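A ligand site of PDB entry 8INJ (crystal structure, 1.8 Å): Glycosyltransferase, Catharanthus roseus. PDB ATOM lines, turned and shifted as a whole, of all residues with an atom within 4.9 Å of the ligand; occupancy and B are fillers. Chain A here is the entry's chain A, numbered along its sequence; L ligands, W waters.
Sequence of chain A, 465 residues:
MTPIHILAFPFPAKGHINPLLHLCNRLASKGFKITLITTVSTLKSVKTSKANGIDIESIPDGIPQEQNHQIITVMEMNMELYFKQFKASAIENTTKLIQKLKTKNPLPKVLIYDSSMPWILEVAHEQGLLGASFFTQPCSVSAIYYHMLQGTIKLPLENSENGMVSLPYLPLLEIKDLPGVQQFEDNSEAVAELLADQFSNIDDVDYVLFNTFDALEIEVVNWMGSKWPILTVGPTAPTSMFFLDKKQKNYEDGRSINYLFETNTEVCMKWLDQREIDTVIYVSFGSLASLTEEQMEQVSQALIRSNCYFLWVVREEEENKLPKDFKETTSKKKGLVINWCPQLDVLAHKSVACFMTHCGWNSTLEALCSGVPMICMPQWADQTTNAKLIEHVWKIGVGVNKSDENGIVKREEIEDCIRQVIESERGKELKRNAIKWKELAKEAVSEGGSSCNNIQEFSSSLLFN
N2 of the ligand lies close to NE1 of Trp 340 (3.5 Å).
Residues that only touch the ligand: Val 313, Gly 15, Gly 360, Ser 284, Tyr 282, Gly 286 and Leu 288.
Hydrophobic or aromatic side chains that line the ligand: Val 313, Trp 340 and His 358.
17 residues have an atom within 4 Å of the ligand: Gly 15, Asn 18, Tyr 282, Ser 284, Gly 286, Ser 287, Leu 288, Val 313, Trp 340, Cys 341, Gln 343, His 358, Gly 360, Trp 361, Asn 362, Ser 363 and Glu 366.
Water W6 lies within hydrogen-bond range of an oxygen (O10) of the ligand (2.7 Å), the backbone NH of Gly 15 (2.8 Å) and the side-chain hydroxyl of Ser 287 (3.2 Å).
Water W5 lies within hydrogen-bond range of O11 of the ligand (2.7 Å), N of Leu 288 (2.9 Å), NE2 of His 358 (3.3 Å) and N of Ser 287 (3.4 Å).
Water W1 lies within hydrogen-bond range of the side-chain carboxylate (OE2) of Glu 366 (2.7 Å) and an oxygen (O5) of the ligand (2.8 Å).
Water W7 lies within hydrogen-bond range of an oxygen (O1) of the ligand (3.0 Å), the indole nitrogen (NE1) of Trp 340 (3.0 Å) and the side-chain amide nitrogen (ND2) of Asn 18 (3.1 Å).
Water W4 lies within hydrogen-bond range of OG of Ser 284, NE2 of Gln 343 and OG of Ser 363.
OE1 of Gln 343 sits at hydrogen-bond distance from OG of Ser 363, at 3.1 Å.
The side-chain sulfur (SG) of Cys 341 sits close to the backbone NH (N) of Gln 343 (3.8 Å).
SG of Cys 341 lies within hydrogen-bond range of OH of Tyr 282, at 3.1 Å.
The side-chain carboxylate (OE1) of Glu 366 sits close to the side-chain amide oxygen (OE1) of Gln 343, 2.8 Å away.
O of Gly 15 lies within hydrogen-bond range of ND2 of Asn 362 (2.8 Å).
The side-chain amide nitrogen (NE2) of Gln 343 is in hydrogen-bond range of the side-chain hydroxyl (OH) of Tyr 282 (2.7 Å).
OG of Ser 284 is in hydrogen-bond range of N of Gly 286, at 3.1 Å.
N of Ser 287 lies within hydrogen-bond range of O12 of the ligand (2.8 Å).
OG of Ser 287 lies within hydrogen-bond range of O12 of the ligand, at 2.6 Å.
An oxygen (O8) of the ligand lies within hydrogen-bond range of the backbone NH (N) of Ser 363.
The side-chain hydroxyl (OG) of Ser 363 sits at hydrogen-bond distance from an oxygen (O8) of the ligand (2.6 Å).
An oxygen (O2) of the ligand lies within hydrogen-bond range of the backbone NH (N) of Cys 341 (2.8 Å).
The backbone carbonyl oxygen (O) of Cys 341 sits at hydrogen-bond distance from a nitrogen (N2) of the ligand (2.8 Å).
The side-chain sulfur (SG) of Cys 341 sits at hydrogen-bond distance from an oxygen (O2) of the ligand, 3.4 Å away.
OE1 of Glu 366 is in hydrogen-bond range of O3 of the ligand, at 2.8 Å.
The backbone NH (N) of Asn 362 sits at hydrogen-bond distance from an oxygen (O7) of the ligand.
An oxygen (O7) of the ligand is in hydrogen-bond range of the side-chain amide nitrogen (ND2) of Asn 362 (2.8 Å).
NE2 of His 358 lies within hydrogen-bond range of O9 of the ligand.
The side-chain amide nitrogen of Asn 18 lies within hydrogen-bond range of an oxygen (O5) of the ligand.
The side-chain amide oxygen (OE1) of Gln 343 sits at hydrogen-bond distance from an oxygen (O3) of the ligand (3.3 Å).
The backbone NH (N) of Trp 361 sits at hydrogen-bond distance from an oxygen (O7) of the ligand (3.4 Å).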
ATOM      1  N   LYS A  14      18.844   1.846  36.411  1.00  0.00           N
ATOM      2  CA  LYS A  14      17.611   1.608  35.660  1.00  0.00           C
ATOM      3  C   LYS A  14      17.836   0.751  34.410  1.00  0.00           C
ATOM      4  O   LYS A  14      16.981  -0.057  34.055  1.00  0.00           O
ATOM      5  CB  LYS A  14      16.946   2.939  35.296  1.00  0.00           C
ATOM      6  CG  LYS A  14      16.369   3.626  36.535  1.00  0.00           C
ATOM      7  CD  LYS A  14      15.361   4.702  36.185  1.00  0.00           C
ATOM      8  CE  LYS A  14      14.858   5.415  37.431  1.00  0.00           C
ATOM      9  NZ  LYS A  14      15.979   5.777  38.375  1.00  0.00           N
ATOM     10  N   GLY A  15      18.976   0.925  33.728  1.00  0.00           N
ATOM     11  CA  GLY A  15      19.257   0.105  32.562  1.00  0.00           C
ATOM     12  C   GLY A  15      19.579  -1.355  32.888  1.00  0.00           C
ATOM     13  O   GLY A  15      19.709  -2.168  31.972  1.00  0.00           O
ATOM     14  N   ASN A  18      15.381  -2.447  34.515  1.00  0.00           N
ATOM     15  CA  ASN A  18      14.269  -2.571  33.594  1.00  0.00           C
ATOM     16  C   ASN A  18      14.303  -3.842  32.740  1.00  0.00           C
ATOM     17  O   ASN A  18      13.273  -4.534  32.671  1.00  0.00           O
ATOM     18  CB  ASN A  18      14.194  -1.309  32.720  1.00  0.00           C
ATOM     19  CG  ASN A  18      13.739  -0.105  33.520  1.00  0.00           C
ATOM     20  OD1 ASN A  18      13.325  -0.217  34.672  1.00  0.00           O
ATOM     21  ND2 ASN A  18      13.793   1.083  32.895  1.00  0.00           N
ATOM     22  N   TYR A 259       6.503  -0.407  34.045  1.00  0.00           N
ATOM     23  CA  TYR A 259       7.406   0.602  34.631  1.00  0.00           C
ATOM     24  C   TYR A 259       7.319   0.613  36.164  1.00  0.00           C
ATOM     25  O   TYR A 259       6.215   0.471  36.703  1.00  0.00           O
ATOM     26  CB  TYR A 259       7.059   1.998  34.106  1.00  0.00           C
ATOM     27  CG  TYR A 259       6.951   2.119  32.606  1.00  0.00           C
ATOM     28  CD1 TYR A 259       8.091   2.182  31.814  1.00  0.00           C
ATOM     29  CD2 TYR A 259       5.713   2.184  31.987  1.00  0.00           C
ATOM     30  CE1 TYR A 259       7.998   2.295  30.445  1.00  0.00           C
ATOM     31  CE2 TYR A 259       5.610   2.296  30.610  1.00  0.00           C
ATOM     32  CZ  TYR A 259       6.758   2.348  29.831  1.00  0.00           C
ATOM     33  OH  TYR A 259       6.665   2.470  28.485  1.00  0.00           O
ATOM     34  N   TYR A 282      12.600  12.229  19.397  1.00  0.00           N
ATOM     35  CA  TYR A 282      12.704  11.847  20.791  1.00  0.00           C
ATOM     36  C   TYR A 282      14.165  11.934  21.208  1.00  0.00           C
ATOM     37  O   TYR A 282      15.036  11.467  20.468  1.00  0.00           O
ATOM     38  CB  TYR A 282      12.150  10.444  20.993  1.00  0.00           C
ATOM     39  CG  TYR A 282      12.345   9.871  22.369  1.00  0.00           C
ATOM     40  CD1 TYR A 282      12.061  10.615  23.515  1.00  0.00           C
ATOM     41  CD2 TYR A 282      12.789   8.567  22.516  1.00  0.00           C
ATOM     42  CE1 TYR A 282      12.228  10.065  24.797  1.00  0.00           C
ATOM     43  CE2 TYR A 282      12.970   8.022  23.779  1.00  0.00           C
ATOM     44  CZ  TYR A 282      12.687   8.769  24.912  1.00  0.00           C
ATOM     45  OH  TYR A 282      12.865   8.200  26.171  1.00  0.00           O
ATOM     46  N   SER A 284      16.928  11.395  24.448  1.00  0.00           N
ATOM     47  CA  SER A 284      17.172  10.946  25.812  1.00  0.00           C
ATOM     48  C   SER A 284      18.602  10.446  25.919  1.00  0.00           C
ATOM     49  O   SER A 284      19.084   9.741  25.032  1.00  0.00           O
ATOM     50  CB  SER A 284      16.206   9.843  26.227  1.00  0.00           C
ATOM     51  OG  SER A 284      16.595   9.303  27.480  1.00  0.00           O
ATOM     52  N   GLY A 286      19.431   8.638  28.670  1.00  0.00           N
ATOM     53  CA  GLY A 286      19.367   7.537  29.582  1.00  0.00           C
ATOM     54  C   GLY A 286      19.230   7.964  31.035  1.00  0.00           C
ATOM     55  O   GLY A 286      18.775   9.065  31.381  1.00  0.00           O
ATOM     56  N   SER A 287      19.630   7.041  31.906  1.00  0.00           N
ATOM     57  CA  SER A 287      19.420   7.152  33.339  1.00  0.00           C
ATOM     58  C   SER A 287      20.658   7.592  34.100  1.00  0.00           C
ATOM     59  O   SER A 287      20.540   7.964  35.274  1.00  0.00           O
ATOM     60  CB  SER A 287      18.911   5.810  33.887  1.00  0.00           C
ATOM     61  OG  SER A 287      19.948   4.825  33.944  1.00  0.00           O
ATOM     62  N   LEU A 288      21.831   7.584  33.459  1.00  0.00           N
ATOM     63  CA  LEU A 288      23.100   7.809  34.134  1.00  0.00           C
ATOM     64  C   LEU A 288      23.908   8.955  33.533  1.00  0.00           C
ATOM     65  O   LEU A 288      24.450   9.769  34.284  1.00  0.00           O
ATOM     66  CB  LEU A 288      23.946   6.529  34.087  1.00  0.00           C
ATOM     67  CG  LEU A 288      23.407   5.326  34.848  1.00  0.00           C
ATOM     68  CD1 LEU A 288      24.267   4.087  34.593  1.00  0.00           C
ATOM     69  CD2 LEU A 288      23.309   5.638  36.339  1.00  0.00           C
ATOM     70  N   VAL A 313      13.882  14.121  27.236  1.00  0.00           N
ATOM     71  CA  VAL A 313      14.000  13.724  28.637  1.00  0.00           C
ATOM     72  C   VAL A 313      15.259  14.357  29.228  1.00  0.00           C
ATOM     73  O   VAL A 313      16.381  14.048  28.802  1.00  0.00           O
ATOM     74  CB  VAL A 313      14.038  12.201  28.782  1.00  0.00           C
ATOM     75  CG1 VAL A 313      14.252  11.821  30.254  1.00  0.00           C
ATOM     76  CG2 VAL A 313      12.747  11.593  28.262  1.00  0.00           C
ATOM     77  N   TRP A 340      11.240  12.365  32.841  1.00  0.00           N
ATOM     78  CA  TRP A 340      11.226  10.934  32.555  1.00  0.00           C
ATOM     79  C   TRP A 340       9.971  10.633  31.748  1.00  0.00           C
ATOM     80  O   TRP A 340       8.935  11.278  31.970  1.00  0.00           O
ATOM     81  CB  TRP A 340      11.240  10.104  33.855  1.00  0.00           C
ATOM     82  CG  TRP A 340      11.867   8.715  33.724  1.00  0.00           C
ATOM     83  CD1 TRP A 340      11.247   7.511  33.934  1.00  0.00           C
ATOM     84  CD2 TRP A 340      13.222   8.407  33.368  1.00  0.00           C
ATOM     85  NE1 TRP A 340      12.131   6.473  33.735  1.00  0.00           N
ATOM     86  CE2 TRP A 340      13.354   6.999  33.377  1.00  0.00           C
ATOM     87  CE3 TRP A 340      14.337   9.179  33.042  1.00  0.00           C
ATOM     88  CZ2 TRP A 340      14.560   6.352  33.088  1.00  0.00           C
ATOM     89  CZ3 TRP A 340      15.545   8.534  32.740  1.00  0.00           C
ATOM     90  CH2 TRP A 340      15.630   7.139  32.759  1.00  0.00           C
ATOM     91  N   CYS A 341      10.019   9.690  30.817  1.00  0.00           N
ATOM     92  CA  CYS A 341       8.882   9.371  29.979  1.00  0.00           C
ATOM     93  C   CYS A 341       8.680   7.866  29.954  1.00  0.00           C
ATOM     94  O   CYS A 341       9.514   7.108  30.455  1.00  0.00           O
ATOM     95  CB  CYS A 341       9.088   9.931  28.555  1.00  0.00           C
ATOM     96  SG  CYS A 341      10.141   8.880  27.488  1.00  0.00           S
ATOM     97  N   PRO A 342       7.530   7.389  29.443  1.00  0.00           N
ATOM     98  CA  PRO A 342       7.389   5.943  29.240  1.00  0.00           C
ATOM     99  C   PRO A 342       8.023   5.517  27.924  1.00  0.00           C
ATOM    100  O   PRO A 342       7.354   5.500  26.870  1.00  0.00           O
ATOM    101  CB  PRO A 342       5.875   5.735  29.267  1.00  0.00           C
ATOM    102  CG  PRO A 342       5.323   7.017  28.686  1.00  0.00           C
ATOM    103  CD  PRO A 342       6.283   8.122  29.127  1.00  0.00           C
ATOM    104  N   GLN A 343       9.315   5.202  27.971  1.00  0.00           N
ATOM    105  CA  GLN A 343      10.115   5.140  26.745  1.00  0.00           C
ATOM    106  C   GLN A 343       9.557   4.107  25.772  1.00  0.00           C
ATOM    107  O   GLN A 343       9.570   4.330  24.562  1.00  0.00           O
ATOM    108  CB  GLN A 343      11.590   4.849  27.062  1.00  0.00           C
ATOM    109  CG  GLN A 343      12.410   4.602  25.781  1.00  0.00           C
ATOM    110  CD  GLN A 343      13.911   4.749  25.931  1.00  0.00           C
ATOM    111  OE1 GLN A 343      14.681   3.808  25.654  1.00  0.00           O
ATOM    112  NE2 GLN A 343      14.350   5.906  26.383  1.00  0.00           N
ATOM    113  N   LEU A 344       9.080   2.956  26.274  1.00  0.00           N
ATOM    114  CA  LEU A 344       8.514   1.955  25.362  1.00  0.00           C
ATOM    115  C   LEU A 344       7.313   2.521  24.622  1.00  0.00           C
ATOM    116  O   LEU A 344       7.157   2.301  23.418  1.00  0.00           O
ATOM    117  CB  LEU A 344       8.114   0.683  26.106  1.00  0.00           C
ATOM    118  CG  LEU A 344       9.178  -0.052  26.918  1.00  0.00           C
ATOM    119  CD1 LEU A 344       8.577  -1.298  27.535  1.00  0.00           C
ATOM    120  CD2 LEU A 344      10.345  -0.394  26.038  1.00  0.00           C
ATOM    121  N   HIS A 358      21.951   8.294  23.578  1.00  0.00           N
ATOM    122  CA  HIS A 358      23.313   7.993  24.017  1.00  0.00           C
ATOM    123  C   HIS A 358      23.748   6.578  23.664  1.00  0.00           C
ATOM    124  O   HIS A 358      24.908   6.221  23.919  1.00  0.00           O
ATOM    125  CB  HIS A 358      23.437   8.200  25.540  1.00  0.00           C
ATOM    126  CG  HIS A 358      22.853   7.092  26.367  1.00  0.00           C
ATOM    127  ND1 HIS A 358      21.561   6.631  26.194  1.00  0.00           N
ATOM    128  CD2 HIS A 358      23.362   6.397  27.408  1.00  0.00           C
ATOM    129  CE1 HIS A 358      21.317   5.680  27.071  1.00  0.00           C
ATOM    130  NE2 HIS A 358      22.393   5.519  27.829  1.00  0.00           N
ATOM    131  N   GLY A 360      22.822   3.574  24.909  1.00  0.00           N
ATOM    132  CA  GLY A 360      22.759   2.463  25.855  1.00  0.00           C
ATOM    133  C   GLY A 360      22.019   1.297  25.235  1.00  0.00           C
ATOM    134  O   GLY A 360      21.200   1.468  24.322  1.00  0.00           O
ATOM    135  N   TRP A 361      22.315   0.076  25.695  1.00  0.00           N
ATOM    136  CA  TRP A 361      21.786  -1.077  24.966  1.00  0.00           C
ATOM    137  C   TRP A 361      20.254  -1.139  25.028  1.00  0.00           C
ATOM    138  O   TRP A 361      19.617  -1.507  24.032  1.00  0.00           O
ATOM    139  CB  TRP A 361      22.386  -2.398  25.468  1.00  0.00           C
ATOM    140  CG  TRP A 361      21.838  -3.560  24.685  1.00  0.00           C
ATOM    141  CD1 TRP A 361      21.209  -4.667  25.190  1.00  0.00           C
ATOM    142  CD2 TRP A 361      21.885  -3.742  23.251  1.00  0.00           C
ATOM    143  NE1 TRP A 361      20.835  -5.510  24.159  1.00  0.00           N
ATOM    144  CE2 TRP A 361      21.246  -4.964  22.959  1.00  0.00           C
ATOM    145  CE3 TRP A 361      22.385  -2.968  22.190  1.00  0.00           C
ATOM    146  CZ2 TRP A 361      21.108  -5.453  21.657  1.00  0.00           C
ATOM    147  CZ3 TRP A 361      22.236  -3.458  20.880  1.00  0.00           C
ATOM    148  CH2 TRP A 361      21.604  -4.683  20.624  1.00  0.00           C
ATOM    149  N   ASN A 362      19.631  -0.831  26.175  1.00  0.00           N
ATOM    150  CA  ASN A 362      18.176  -0.913  26.200  1.00  0.00           C
ATOM    151  C   ASN A 362      17.567   0.037  25.179  1.00  0.00           C
ATOM    152  O   ASN A 362      16.654  -0.323  24.439  1.00  0.00           O
ATOM    153  CB  ASN A 362      17.612  -0.579  27.567  1.00  0.00           C
ATOM    154  CG  ASN A 362      17.992  -1.621  28.583  1.00  0.00           C
ATOM    155  OD1 ASN A 362      17.496  -2.736  28.541  1.00  0.00           O
ATOM    156  ND2 ASN A 362      18.920  -1.268  29.452  1.00  0.00           N
ATOM    157  N   SER A 363      18.066   1.261  25.166  1.00  0.00           N
ATOM    158  CA  SER A 363      17.553   2.251  24.235  1.00  0.00           C
ATOM    159  C   SER A 363      17.767   1.834  22.784  1.00  0.00           C
ATOM    160  O   SER A 363      16.865   1.996  21.932  1.00  0.00           O
ATOM    161  CB  SER A 363      18.220   3.585  24.533  1.00  0.00           C
ATOM    162  OG  SER A 363      17.726   4.102  25.749  1.00  0.00           O
ATOM    163  N   GLU A 366      15.389  -1.169  22.144  1.00  0.00           N
ATOM    164  CA  GLU A 366      13.990  -0.730  22.110  1.00  0.00           C
ATOM    165  C   GLU A 366      13.692   0.063  20.843  1.00  0.00           C
ATOM    166  O   GLU A 366      12.628  -0.091  20.233  1.00  0.00           O
ATOM    167  CB  GLU A 366      13.660   0.066  23.375  1.00  0.00           C
ATOM    168  CG  GLU A 366      13.601  -0.851  24.632  1.00  0.00           C
ATOM    169  CD  GLU A 366      13.772  -0.099  25.934  1.00  0.00           C
ATOM    170  OE1 GLU A 366      13.726   1.152  25.897  1.00  0.00           O
ATOM    171  OE2 GLU A 366      13.963  -0.753  26.994  1.00  0.00           O
ATOM    172  N   TRP A 380      29.959   6.875  26.899  1.00  0.00           N
ATOM    173  CA  TRP A 380      31.008   6.055  27.503  1.00  0.00           C
ATOM    174  C   TRP A 380      30.560   4.604  27.565  1.00  0.00           C
ATOM    175  O   TRP A 380      29.461   4.243  27.121  1.00  0.00           O
ATOM    176  CB  TRP A 380      31.405   6.571  28.896  1.00  0.00           C
ATOM    177  CG  TRP A 380      30.271   7.137  29.713  1.00  0.00           C
ATOM    178  CD1 TRP A 380      30.034   8.453  30.003  1.00  0.00           C
ATOM    179  CD2 TRP A 380      29.224   6.397  30.362  1.00  0.00           C
ATOM    180  NE1 TRP A 380      28.917   8.581  30.783  1.00  0.00           N
ATOM    181  CE2 TRP A 380      28.398   7.330  31.020  1.00  0.00           C
ATOM    182  CE3 TRP A 380      28.908   5.035  30.461  1.00  0.00           C
ATOM    183  CZ2 TRP A 380      27.283   6.951  31.759  1.00  0.00           C
ATOM    184  CZ3 TRP A 380      27.794   4.659  31.187  1.00  0.00           C
ATOM    185  CH2 TRP A 380      26.990   5.615  31.836  1.00  0.00           C
ATOM    186  N   GLN A 383      28.344   2.275  25.009  1.00  0.00           N
ATOM    187  CA  GLN A 383      27.647   3.159  24.075  1.00  0.00           C
ATOM    188  C   GLN A 383      28.445   3.418  22.805  1.00  0.00           C
ATOM    189  O   GLN A 383      27.881   3.536  21.712  1.00  0.00           O
ATOM    190  CB  GLN A 383      27.330   4.484  24.774  1.00  0.00           C
ATOM    191  CG  GLN A 383      26.415   4.308  25.986  1.00  0.00           C
ATOM    192  CD  GLN A 383      26.624   5.379  27.054  1.00  0.00           C
ATOM    193  OE1 GLN A 383      26.972   6.499  26.755  1.00  0.00           O
ATOM    194  NE2 GLN A 383      26.420   5.001  28.311  1.00  0.00           N
HETATM  195  N1  LIG L   1      13.916   5.052  30.047  1.00  0.00           N
HETATM  196  C1  LIG L   1      12.668   5.373  30.345  1.00  0.00           C
HETATM  197  N2  LIG L   1      12.237   6.615  30.283  1.00  0.00           N
HETATM  198  C2  LIG L   1      13.055   7.578  29.915  1.00  0.00           C
HETATM  199  C3  LIG L   1      14.389   7.309  29.592  1.00  0.00           C
HETATM  200  C4  LIG L   1      14.799   5.981  29.682  1.00  0.00           C
HETATM  201  O1  LIG L   1      11.763   4.379  30.712  1.00  0.00           O
HETATM  202  O2  LIG L   1      12.568   8.853  29.874  1.00  0.00           O
HETATM  203  C5  LIG L   1      14.369   3.655  30.196  1.00  0.00           C
HETATM  204  C6  LIG L   1      14.744   2.918  28.910  1.00  0.00           C
HETATM  205  O3  LIG L   1      13.623   2.327  28.413  1.00  0.00           O
HETATM  206  C7  LIG L   1      15.727   1.862  29.484  1.00  0.00           C
HETATM  207  C8  LIG L   1      16.435   2.507  30.394  1.00  0.00           C
HETATM  208  O4  LIG L   1      15.487   3.676  30.908  1.00  0.00           O
HETATM  209  O5  LIG L   1      14.929   0.787  30.153  1.00  0.00           O
HETATM  210  C9  LIG L   1      17.666   3.142  29.758  1.00  0.00           C
HETATM  211  O6  LIG L   1      18.621   2.115  29.684  1.00  0.00           O
HETATM  212  P1  LIG L   1      19.893   2.213  28.661  1.00  0.00           P
HETATM  213  O7  LIG L   1      20.512   0.857  28.490  1.00  0.00           O
HETATM  214  O8  LIG L   1      19.380   2.756  27.315  1.00  0.00           O
HETATM  215  O9  LIG L   1      20.945   3.353  29.176  1.00  0.00           O
HETATM  216  P2  LIG L   1      21.491   3.610  30.706  1.00  0.00           P
HETATM  217  O10 LIG L   1      21.713   2.262  31.383  1.00  0.00           O
HETATM  218  O11 LIG L   1      22.762   4.371  30.505  1.00  0.00           O
HETATM  219  O12 LIG L   1      20.458   4.400  31.476  1.00  0.00           O
HETATM  220  O   HOH W   1      12.631  -0.524  29.364  1.00  0.00           O
HETATM  221  O   HOH W   2      11.080   1.594  29.952  1.00  0.00           O
HETATM  222  O   HOH W   3      25.056   2.771  31.135  1.00  0.00           O
HETATM  223  O   HOH W   4      16.868   6.665  27.158  1.00  0.00           O
HETATM  224  O   HOH W   5      22.775   7.030  30.735  1.00  0.00           O
HETATM  225  O   HOH W   6      21.509   2.036  34.018  1.00  0.00           O
HETATM  226  O   HOH W   7      11.950   3.466  33.562  1.00  0.00           O
